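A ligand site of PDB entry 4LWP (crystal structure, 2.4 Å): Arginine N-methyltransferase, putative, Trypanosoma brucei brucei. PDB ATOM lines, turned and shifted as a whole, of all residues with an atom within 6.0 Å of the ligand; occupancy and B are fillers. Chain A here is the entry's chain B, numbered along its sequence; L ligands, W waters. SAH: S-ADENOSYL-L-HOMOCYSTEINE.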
ATOM      1  N   HIS A  30     -15.804  21.518 -18.412  1.00  0.00           N
ATOM      2  CA  HIS A  30     -15.849  21.847 -19.833  1.00  0.00           C
ATOM      3  C   HIS A  30     -15.427  23.284 -20.054  1.00  0.00           C
ATOM      4  O   HIS A  30     -14.774  23.606 -21.053  1.00  0.00           O
ATOM      5  CB  HIS A  30     -17.236  21.580 -20.427  1.00  0.00           C
ATOM      6  CG  HIS A  30     -17.508  20.118 -20.630  1.00  0.00           C
ATOM      7  ND1 HIS A  30     -17.286  19.484 -21.839  1.00  0.00           N
ATOM      8  CD2 HIS A  30     -17.938  19.157 -19.783  1.00  0.00           C
ATOM      9  CE1 HIS A  30     -17.574  18.202 -21.713  1.00  0.00           C
ATOM     10  NE2 HIS A  30     -17.972  17.979 -20.483  1.00  0.00           N
ATOM     11  N   MET A  33     -11.761  23.447 -20.302  1.00  0.00           N
ATOM     12  CA  MET A  33     -11.289  23.022 -21.623  1.00  0.00           C
ATOM     13  C   MET A  33     -11.563  24.083 -22.676  1.00  0.00           C
ATOM     14  O   MET A  33     -10.784  24.251 -23.605  1.00  0.00           O
ATOM     15  CB  MET A  33     -11.954  21.696 -22.003  1.00  0.00           C
ATOM     16  CG  MET A  33     -11.571  20.524 -21.115  1.00  0.00           C
ATOM     17  SD  MET A  33     -12.267  18.942 -21.662  1.00  0.00           S
ATOM     18  CE  MET A  33     -14.000  19.351 -21.731  1.00  0.00           C
ATOM     19  N   LEU A  34     -12.670  24.815 -22.534  1.00  0.00           N
ATOM     20  CA  LEU A  34     -12.989  25.871 -23.480  1.00  0.00           C
ATOM     21  C   LEU A  34     -12.123  27.113 -23.291  1.00  0.00           C
ATOM     22  O   LEU A  34     -11.951  27.878 -24.231  1.00  0.00           O
ATOM     23  CB  LEU A  34     -14.451  26.278 -23.341  1.00  0.00           C
ATOM     24  CG  LEU A  34     -15.484  25.223 -23.711  1.00  0.00           C
ATOM     25  CD1 LEU A  34     -16.854  25.691 -23.256  1.00  0.00           C
ATOM     26  CD2 LEU A  34     -15.445  25.011 -25.216  1.00  0.00           C
ATOM     27  N   ARG A  39      -5.636  24.662 -26.937  1.00  0.00           N
ATOM     28  CA  ARG A  39      -6.496  23.549 -27.297  1.00  0.00           C
ATOM     29  C   ARG A  39      -7.544  24.010 -28.315  1.00  0.00           C
ATOM     30  O   ARG A  39      -7.699  23.422 -29.377  1.00  0.00           O
ATOM     31  CB  ARG A  39      -7.170  22.980 -26.055  1.00  0.00           C
ATOM     32  CG  ARG A  39      -7.906  21.686 -26.271  1.00  0.00           C
ATOM     33  CD  ARG A  39      -8.815  21.341 -25.091  1.00  0.00           C
ATOM     34  NE  ARG A  39     -10.101  22.037 -25.194  1.00  0.00           N
ATOM     35  CZ  ARG A  39     -11.238  21.463 -25.595  1.00  0.00           C
ATOM     36  NH1 ARG A  39     -11.257  20.173 -25.941  1.00  0.00           N
ATOM     37  NH2 ARG A  39     -12.355  22.181 -25.671  1.00  0.00           N
ATOM     38  N   MET A  40      -8.220  25.101 -27.994  1.00  0.00           N
ATOM     39  CA  MET A  40      -9.261  25.616 -28.871  1.00  0.00           C
ATOM     40  C   MET A  40      -8.721  25.989 -30.229  1.00  0.00           C
ATOM     41  O   MET A  40      -9.334  25.716 -31.257  1.00  0.00           O
ATOM     42  CB  MET A  40      -9.925  26.833 -28.230  1.00  0.00           C
ATOM     43  CG  MET A  40     -10.642  26.487 -26.935  1.00  0.00           C
ATOM     44  SD  MET A  40     -12.105  25.488 -27.288  1.00  0.00           S
ATOM     45  CE  MET A  40     -13.183  26.870 -27.757  1.00  0.00           C
ATOM     46  N   TYR A  43      -7.939  22.954 -32.733  1.00  0.00           N
ATOM     47  CA  TYR A  43      -9.134  22.359 -33.340  1.00  0.00           C
ATOM     48  C   TYR A  43      -9.829  23.317 -34.315  1.00  0.00           C
ATOM     49  O   TYR A  43     -10.243  22.884 -35.402  1.00  0.00           O
ATOM     50  CB  TYR A  43     -10.115  21.874 -32.240  1.00  0.00           C
ATOM     51  CG  TYR A  43      -9.723  20.508 -31.696  1.00  0.00           C
ATOM     52  CD1 TYR A  43     -10.067  19.338 -32.376  1.00  0.00           C
ATOM     53  CD2 TYR A  43      -8.925  20.390 -30.553  1.00  0.00           C
ATOM     54  CE1 TYR A  43      -9.686  18.084 -31.920  1.00  0.00           C
ATOM     55  CE2 TYR A  43      -8.519  19.142 -30.082  1.00  0.00           C
ATOM     56  CZ  TYR A  43      -8.900  17.988 -30.770  1.00  0.00           C
ATOM     57  OH  TYR A  43      -8.515  16.742 -30.318  1.00  0.00           O
ATOM     58  N   ASP A  60     -18.517  13.548 -34.346  1.00  0.00           N
ATOM     59  CA  ASP A  60     -17.820  14.096 -33.187  1.00  0.00           C
ATOM     60  C   ASP A  60     -17.975  13.136 -32.005  1.00  0.00           C
ATOM     61  O   ASP A  60     -19.070  12.950 -31.473  1.00  0.00           O
ATOM     62  CB  ASP A  60     -18.347  15.505 -32.867  1.00  0.00           C
ATOM     63  CG  ASP A  60     -17.590  16.192 -31.732  1.00  0.00           C
ATOM     64  OD1 ASP A  60     -16.579  15.628 -31.207  1.00  0.00           O
ATOM     65  OD2 ASP A  60     -18.003  17.314 -31.361  1.00  0.00           O
ATOM     66  N   VAL A  61     -16.879  12.478 -31.636  1.00  0.00           N
ATOM     67  CA  VAL A  61     -16.888  11.479 -30.575  1.00  0.00           C
ATOM     68  C   VAL A  61     -16.516  12.087 -29.228  1.00  0.00           C
ATOM     69  O   VAL A  61     -15.371  12.505 -29.024  1.00  0.00           O
ATOM     70  CB  VAL A  61     -15.909  10.321 -30.864  1.00  0.00           C
ATOM     71  CG1 VAL A  61     -15.919   9.295 -29.752  1.00  0.00           C
ATOM     72  CG2 VAL A  61     -16.269   9.666 -32.134  1.00  0.00           C
ATOM     73  N   GLY A  62     -17.479  12.129 -28.302  1.00  0.00           N
ATOM     74  CA  GLY A  62     -17.279  12.777 -27.013  1.00  0.00           C
ATOM     75  C   GLY A  62     -17.378  14.290 -27.134  1.00  0.00           C
ATOM     76  O   GLY A  62     -16.465  15.020 -26.744  1.00  0.00           O
ATOM     77  N   SER A  63     -18.501  14.743 -27.656  1.00  0.00           N
ATOM     78  CA  SER A  63     -18.684  16.121 -28.091  1.00  0.00           C
ATOM     79  C   SER A  63     -18.907  17.154 -26.958  1.00  0.00           C
ATOM     80  O   SER A  63     -18.777  18.349 -27.197  1.00  0.00           O
ATOM     81  CB  SER A  63     -19.851  16.169 -29.072  1.00  0.00           C
ATOM     82  OG  SER A  63     -21.021  15.611 -28.490  1.00  0.00           O
ATOM     83  N   GLY A  64     -19.278  16.676 -25.766  1.00  0.00           N
ATOM     84  CA  GLY A  64     -19.426  17.547 -24.615  1.00  0.00           C
ATOM     85  C   GLY A  64     -20.380  18.703 -24.819  1.00  0.00           C
ATOM     86  O   GLY A  64     -21.594  18.498 -24.910  1.00  0.00           O
ATOM     87  N   THR A  65     -19.851  19.906 -24.931  1.00  0.00           N
ATOM     88  CA  THR A  65     -20.660  21.082 -25.199  1.00  0.00           C
ATOM     89  C   THR A  65     -21.047  21.157 -26.669  1.00  0.00           C
ATOM     90  O   THR A  65     -21.873  21.993 -27.059  1.00  0.00           O
ATOM     91  CB  THR A  65     -19.948  22.389 -24.780  1.00  0.00           C
ATOM     92  OG1 THR A  65     -18.746  22.549 -25.536  1.00  0.00           O
ATOM     93  CG2 THR A  65     -19.660  22.384 -23.262  1.00  0.00           C
ATOM     94  N   GLY A  66     -20.404  20.348 -27.502  1.00  0.00           N
ATOM     95  CA  GLY A  66     -20.731  20.295 -28.919  1.00  0.00           C
ATOM     96  C   GLY A  66     -19.961  21.308 -29.748  1.00  0.00           C
ATOM     97  O   GLY A  66     -20.225  21.484 -30.941  1.00  0.00           O
ATOM     98  N   ILE A  67     -18.973  21.935 -29.114  1.00  0.00           N
ATOM     99  CA  ILE A  67     -18.175  22.954 -29.778  1.00  0.00           C
ATOM    100  C   ILE A  67     -17.563  22.475 -31.118  1.00  0.00           C
ATOM    101  O   ILE A  67     -17.714  23.156 -32.133  1.00  0.00           O
ATOM    102  CB  ILE A  67     -17.057  23.454 -28.828  1.00  0.00           C
ATOM    103  CG1 ILE A  67     -16.179  24.478 -29.529  1.00  0.00           C
ATOM    104  CG2 ILE A  67     -16.217  22.308 -28.308  1.00  0.00           C
ATOM    105  CD1 ILE A  67     -16.895  25.751 -29.825  1.00  0.00           C
ATOM    106  N   LEU A  68     -16.923  21.304 -31.130  1.00  0.00           N
ATOM    107  CA  LEU A  68     -16.354  20.780 -32.373  1.00  0.00           C
ATOM    108  C   LEU A  68     -17.423  20.446 -33.407  1.00  0.00           C
ATOM    109  O   LEU A  68     -17.214  20.648 -34.597  1.00  0.00           O
ATOM    110  CB  LEU A  68     -15.486  19.541 -32.126  1.00  0.00           C
ATOM    111  CG  LEU A  68     -14.057  19.626 -31.576  1.00  0.00           C
ATOM    112  CD1 LEU A  68     -13.777  20.843 -30.773  1.00  0.00           C
ATOM    113  CD2 LEU A  68     -13.713  18.356 -30.800  1.00  0.00           C
ATOM    114  N   ILE A  83     -21.791  12.776 -30.601  1.00  0.00           N
ATOM    115  CA  ILE A  83     -21.954  11.698 -29.657  1.00  0.00           C
ATOM    116  C   ILE A  83     -21.460  12.104 -28.278  1.00  0.00           C
ATOM    117  O   ILE A  83     -20.296  12.493 -28.121  1.00  0.00           O
ATOM    118  CB  ILE A  83     -21.206  10.441 -30.119  1.00  0.00           C
ATOM    119  CG1 ILE A  83     -21.629  10.044 -31.536  1.00  0.00           C
ATOM    120  CG2 ILE A  83     -21.434   9.277 -29.147  1.00  0.00           C
ATOM    121  CD1 ILE A  83     -20.859   8.834 -32.059  1.00  0.00           C
ATOM    122  N   GLU A  84     -22.347  12.028 -27.285  1.00  0.00           N
ATOM    123  CA  GLU A  84     -22.014  12.381 -25.913  1.00  0.00           C
ATOM    124  C   GLU A  84     -22.835  11.552 -24.932  1.00  0.00           C
ATOM    125  O   GLU A  84     -24.062  11.586 -24.981  1.00  0.00           O
ATOM    126  CB  GLU A  84     -22.249  13.881 -25.653  1.00  0.00           C
ATOM    127  CG  GLU A  84     -22.210  14.272 -24.198  1.00  0.00           C
ATOM    128  CD  GLU A  84     -20.872  13.974 -23.561  1.00  0.00           C
ATOM    129  OE1 GLU A  84     -20.851  13.321 -22.490  1.00  0.00           O
ATOM    130  OE2 GLU A  84     -19.832  14.384 -24.136  1.00  0.00           O
ATOM    131  N   ALA A  85     -22.160  10.824 -24.060  1.00  0.00           N
ATOM    132  CA  ALA A  85     -22.821   9.890 -23.138  1.00  0.00           C
ATOM    133  C   ALA A  85     -23.482  10.565 -21.960  1.00  0.00           C
ATOM    134  O   ALA A  85     -24.446  10.041 -21.394  1.00  0.00           O
ATOM    135  CB  ALA A  85     -21.821   8.883 -22.606  1.00  0.00           C
ATOM    136  N   SER A  86     -22.969  11.724 -21.563  1.00  0.00           N
ATOM    137  CA  SER A  86     -23.410  12.322 -20.303  1.00  0.00           C
ATOM    138  C   SER A  86     -24.673  13.133 -20.533  1.00  0.00           C
ATOM    139  O   SER A  86     -25.190  13.206 -21.647  1.00  0.00           O
ATOM    140  CB  SER A  86     -22.334  13.215 -19.696  1.00  0.00           C
ATOM    141  OG  SER A  86     -22.346  14.448 -20.361  1.00  0.00           O
ATOM    142  N   LEU A  88     -25.031  16.145 -20.485  1.00  0.00           N
ATOM    143  CA  LEU A  88     -24.766  17.314 -21.317  1.00  0.00           C
ATOM    144  C   LEU A  88     -25.427  17.198 -22.686  1.00  0.00           C
ATOM    145  O   LEU A  88     -25.716  18.217 -23.338  1.00  0.00           O
ATOM    146  CB  LEU A  88     -23.263  17.519 -21.512  1.00  0.00           C
ATOM    147  CG  LEU A  88     -22.614  18.647 -20.735  1.00  0.00           C
ATOM    148  CD1 LEU A  88     -21.149  18.762 -21.108  1.00  0.00           C
ATOM    149  CD2 LEU A  88     -23.343  19.962 -21.032  1.00  0.00           C
ATOM    150  N   ASP A 110     -25.620   8.891 -25.973  1.00  0.00           N
ATOM    151  CA  ASP A 110     -25.339   7.528 -25.528  1.00  0.00           C
ATOM    152  C   ASP A 110     -23.827   7.285 -25.612  1.00  0.00           C
ATOM    153  O   ASP A 110     -23.104   8.089 -26.225  1.00  0.00           O
ATOM    154  CB  ASP A 110     -26.128   6.503 -26.366  1.00  0.00           C
ATOM    155  CG  ASP A 110     -26.475   5.240 -25.575  1.00  0.00           C
ATOM    156  OD1 ASP A 110     -25.898   4.998 -24.480  1.00  0.00           O
ATOM    157  OD2 ASP A 110     -27.341   4.473 -26.025  1.00  0.00           O
ATOM    158  N   THR A 111     -23.349   6.197 -25.014  1.00  0.00           N
ATOM    159  CA  THR A 111     -21.945   5.896 -25.166  1.00  0.00           C
ATOM    160  C   THR A 111     -21.690   5.467 -26.587  1.00  0.00           C
ATOM    161  O   THR A 111     -22.593   4.985 -27.261  1.00  0.00           O
ATOM    162  CB  THR A 111     -21.462   4.786 -24.210  1.00  0.00           C
ATOM    163  OG1 THR A 111     -22.185   3.588 -24.493  1.00  0.00           O
ATOM    164  CG2 THR A 111     -21.681   5.177 -22.720  1.00  0.00           C
ATOM    165  N   VAL A 112     -20.465   5.686 -27.057  1.00  0.00           N
ATOM    166  CA  VAL A 112     -20.009   5.115 -28.318  1.00  0.00           C
ATOM    167  C   VAL A 112     -20.304   3.625 -28.359  1.00  0.00           C
ATOM    168  O   VAL A 112     -20.788   3.096 -29.359  1.00  0.00           O
ATOM    169  CB  VAL A 112     -18.483   5.323 -28.508  1.00  0.00           C
ATOM    170  CG1 VAL A 112     -17.923   4.379 -29.593  1.00  0.00           C
ATOM    171  CG2 VAL A 112     -18.198   6.761 -28.865  1.00  0.00           C
ATOM    172  N   GLU A 113     -20.017   2.945 -27.262  1.00  0.00           N
ATOM    173  CA  GLU A 113     -20.102   1.490 -27.223  1.00  0.00           C
ATOM    174  C   GLU A 113     -21.544   0.994 -27.370  1.00  0.00           C
ATOM    175  O   GLU A 113     -21.786  -0.021 -28.043  1.00  0.00           O
ATOM    176  CB  GLU A 113     -19.478   1.005 -25.940  1.00  0.00           C
ATOM    177  CG  GLU A 113     -17.951   1.185 -25.876  1.00  0.00           C
ATOM    178  CD  GLU A 113     -17.504   2.639 -25.681  1.00  0.00           C
ATOM    179  OE1 GLU A 113     -18.355   3.517 -25.366  1.00  0.00           O
ATOM    180  OE2 GLU A 113     -16.286   2.901 -25.823  1.00  0.00           O
ATOM    181  N   SER A 141     -12.496  14.365 -32.495  1.00  0.00           N
ATOM    182  CA  SER A 141     -12.481  13.935 -31.122  1.00  0.00           C
ATOM    183  C   SER A 141     -11.381  14.626 -30.369  1.00  0.00           C
ATOM    184  O   SER A 141     -10.321  14.963 -30.923  1.00  0.00           O
ATOM    185  CB  SER A 141     -12.306  12.418 -31.034  1.00  0.00           C
ATOM    186  OG  SER A 141     -12.531  12.023 -29.694  1.00  0.00           O
ATOM    187  N   GLU A 142     -11.662  14.853 -29.092  1.00  0.00           N
ATOM    188  CA  GLU A 142     -10.640  15.365 -28.203  1.00  0.00           C
ATOM    189  C   GLU A 142     -10.553  14.417 -27.016  1.00  0.00           C
ATOM    190  O   GLU A 142     -11.265  14.555 -26.016  1.00  0.00           O
ATOM    191  CB  GLU A 142     -10.966  16.790 -27.775  1.00  0.00           C
ATOM    192  CG  GLU A 142      -9.766  17.577 -27.359  1.00  0.00           C
ATOM    193  CD  GLU A 142      -9.293  17.189 -25.995  1.00  0.00           C
ATOM    194  OE1 GLU A 142      -8.522  16.185 -25.904  1.00  0.00           O
ATOM    195  OE2 GLU A 142      -9.703  17.857 -25.019  1.00  0.00           O
ATOM    196  N   MET A 153      -9.769   8.867 -23.459  1.00  0.00           N
ATOM    197  CA  MET A 153     -10.808   8.026 -23.982  1.00  0.00           C
ATOM    198  C   MET A 153     -10.376   7.433 -25.328  1.00  0.00           C
ATOM    199  O   MET A 153     -11.217   7.101 -26.168  1.00  0.00           O
ATOM    200  CB  MET A 153     -12.138   8.790 -24.120  1.00  0.00           C
ATOM    201  CG  MET A 153     -12.067  10.102 -24.868  1.00  0.00           C
ATOM    202  SD  MET A 153     -13.705  10.923 -24.980  1.00  0.00           S
ATOM    203  CE  MET A 153     -14.455   9.942 -26.299  1.00  0.00           C
ATOM    204  N   SER A 156     -12.281   4.419 -26.794  1.00  0.00           N
ATOM    205  CA  SER A 156     -13.595   4.675 -27.389  1.00  0.00           C
ATOM    206  C   SER A 156     -13.481   5.293 -28.783  1.00  0.00           C
ATOM    207  O   SER A 156     -14.339   5.062 -29.632  1.00  0.00           O
ATOM    208  CB  SER A 156     -14.442   5.589 -26.490  1.00  0.00           C
ATOM    209  OG  SER A 156     -14.773   4.944 -25.251  1.00  0.00           O
HETATM  210  N   SAH L   1     -15.431  17.504 -27.499  1.00  0.00           N
HETATM  211  CA  SAH L   1     -15.553  18.405 -26.361  1.00  0.00           C
HETATM  212  CB  SAH L   1     -15.471  17.645 -25.042  1.00  0.00           C
HETATM  213  CG  SAH L   1     -14.418  16.554 -24.908  1.00  0.00           C
HETATM  214  SD  SAH L   1     -14.346  15.963 -23.194  1.00  0.00           S
HETATM  215  C   SAH L   1     -14.486  19.475 -26.461  1.00  0.00           C
HETATM  216  O   SAH L   1     -14.567  20.515 -25.803  1.00  0.00           O
HETATM  217  OXT SAH L   1     -13.516  19.287 -27.213  1.00  0.00           O
HETATM  218  C5' SAH L   1     -14.815  14.296 -23.700  1.00  0.00           C
HETATM  219  C4' SAH L   1     -16.323  14.016 -23.607  1.00  0.00           C
HETATM  220  O4' SAH L   1     -16.551  12.693 -24.055  1.00  0.00           O
HETATM  221  C3' SAH L   1     -16.964  14.106 -22.232  1.00  0.00           C
HETATM  222  O3' SAH L   1     -18.062  14.995 -22.304  1.00  0.00           O
HETATM  223  C2' SAH L   1     -17.482  12.698 -21.940  1.00  0.00           C
HETATM  224  O2' SAH L   1     -18.773  12.679 -21.384  1.00  0.00           O
HETATM  225  C1' SAH L   1     -17.584  12.093 -23.325  1.00  0.00           C
HETATM  226  N9  SAH L   1     -17.315  10.656 -23.419  1.00  0.00           N
HETATM  227  C8  SAH L   1     -16.264   9.971 -22.851  1.00  0.00           C
HETATM  228  N7  SAH L   1     -16.380   8.688 -23.214  1.00  0.00           N
HETATM  229  C5  SAH L   1     -17.464   8.540 -24.018  1.00  0.00           C
HETATM  230  C6  SAH L   1     -18.000   7.433 -24.662  1.00  0.00           C
HETATM  231  N6  SAH L   1     -17.426   6.237 -24.526  1.00  0.00           N
HETATM  232  N1  SAH L   1     -19.136   7.601 -25.430  1.00  0.00           N
HETATM  233  C2  SAH L   1     -19.725   8.854 -25.561  1.00  0.00           C
HETATM  234  N3  SAH L   1     -19.172   9.952 -24.917  1.00  0.00           N
HETATM  235  C4  SAH L   1     -18.061   9.779 -24.164  1.00  0.00           C
HETATM  236  O   HOH W   1     -16.963  20.591 -24.335  1.00  0.00           O
HETATM  237  O   HOH W   2     -17.426  18.840 -29.335  1.00  0.00           O
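The side-chain carboxylate (OE1) of Glu 84 is in hydrogen-bond range of an oxygen (O2') of the ligand (2.4 Å).
The guanidinium group of Arg 39 is in salt-bridge range of an oxygen (OXT) of the ligand (2.7 Å).
A nitrogen (N) of the ligand sits at hydrogen-bond distance from the backbone carbonyl oxygen (O) of Gly 62 (2.8 Å).
N of Val 112 sits at hydrogen-bond distance from N1 of the ligand.
The side-chain carboxylate (OE1) of Glu 113 lies within hydrogen-bond range of a nitrogen (N6) of the ligand (3.0 Å).
A nitrogen (N6) of the ligand lies within hydrogen-bond range of the side-chain hydroxyl (OG) of Ser 156, at 3.0 Å.
The backbone NH (N) of Ala 85 lies within hydrogen-bond range of a nitrogen (N3) of the ligand, at 3.2 Å.
NE2 of His 30 lies close to O3' of the ligand (3.5 Å).
N of the ligand sits close to O of Ser 63 (3.5 Å).
O of Glu 84 lies within hydrogen-bond range of N of Asp 110, 3.3 Å away.
OE1 of Glu 84 sits at hydrogen-bond distance from N of Ser 86 (2.8 Å).
The backbone carbonyl oxygen of Met 33 lies within hydrogen-bond range of the guanidinium group of Arg 39 (2.8 Å).
N of Gly 62 is in hydrogen-bond range of O of Ile 83, 2.8 Å away.
OE2 of Glu 113 lies within hydrogen-bond range of OG of Ser 156 (2.6 Å).
The backbone NH (N) of Ser 63 lies within hydrogen-bond range of the backbone carbonyl oxygen (O) of Ile 83, 2.9 Å away.
The side-chain hydroxyl of Ser 86 lies close to the backbone NH of Leu 88 (3.2 Å).
The backbone carbonyl oxygen of Asp 60 sits at hydrogen-bond distance from the backbone NH of Ile 83, at 2.9 Å.
SD of Met 153 sits close to O4' of the ligand (3.5 Å).
Residues that only touch the ligand: Thr 111, Ile 67, Asp 110, Glu 142, Gly 64, Met 33, Leu 68, Ser 86 and Ile 83.
Hydrophobic or aromatic side chains within 4 Å of the ligand: His 30, Met 33, Ile 67, Leu 68, Ile 83, Ala 85, Val 112 and Met 153.
19 residues have an atom within 4 Å of the ligand: His 30, Met 33, Arg 39, Gly 62, Ser 63, Gly 64, Ile 67, Leu 68, Ile 83, Glu 84, Ala 85, Ser 86, Asp 110, Thr 111, Val 112, Glu 113, Glu 142, Met 153 and Ser 156.
Water W1 lies within hydrogen-bond range of a ring nitrogen (ND1) of His 30 (2.7 Å), an oxygen (O) of the ligand (2.8 Å) and the side-chain hydroxyl (OG1) of Thr 65 (2.9 Å).
Water W2 lies within hydrogen-bond range of the backbone carbonyl oxygen (O) of Ser 63, the side-chain carboxylate (OD2) of Asp 60, a nitrogen (N) of the ligand, the backbone NH (N) of Leu 68 and the backbone NH (N) of Ile 67.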
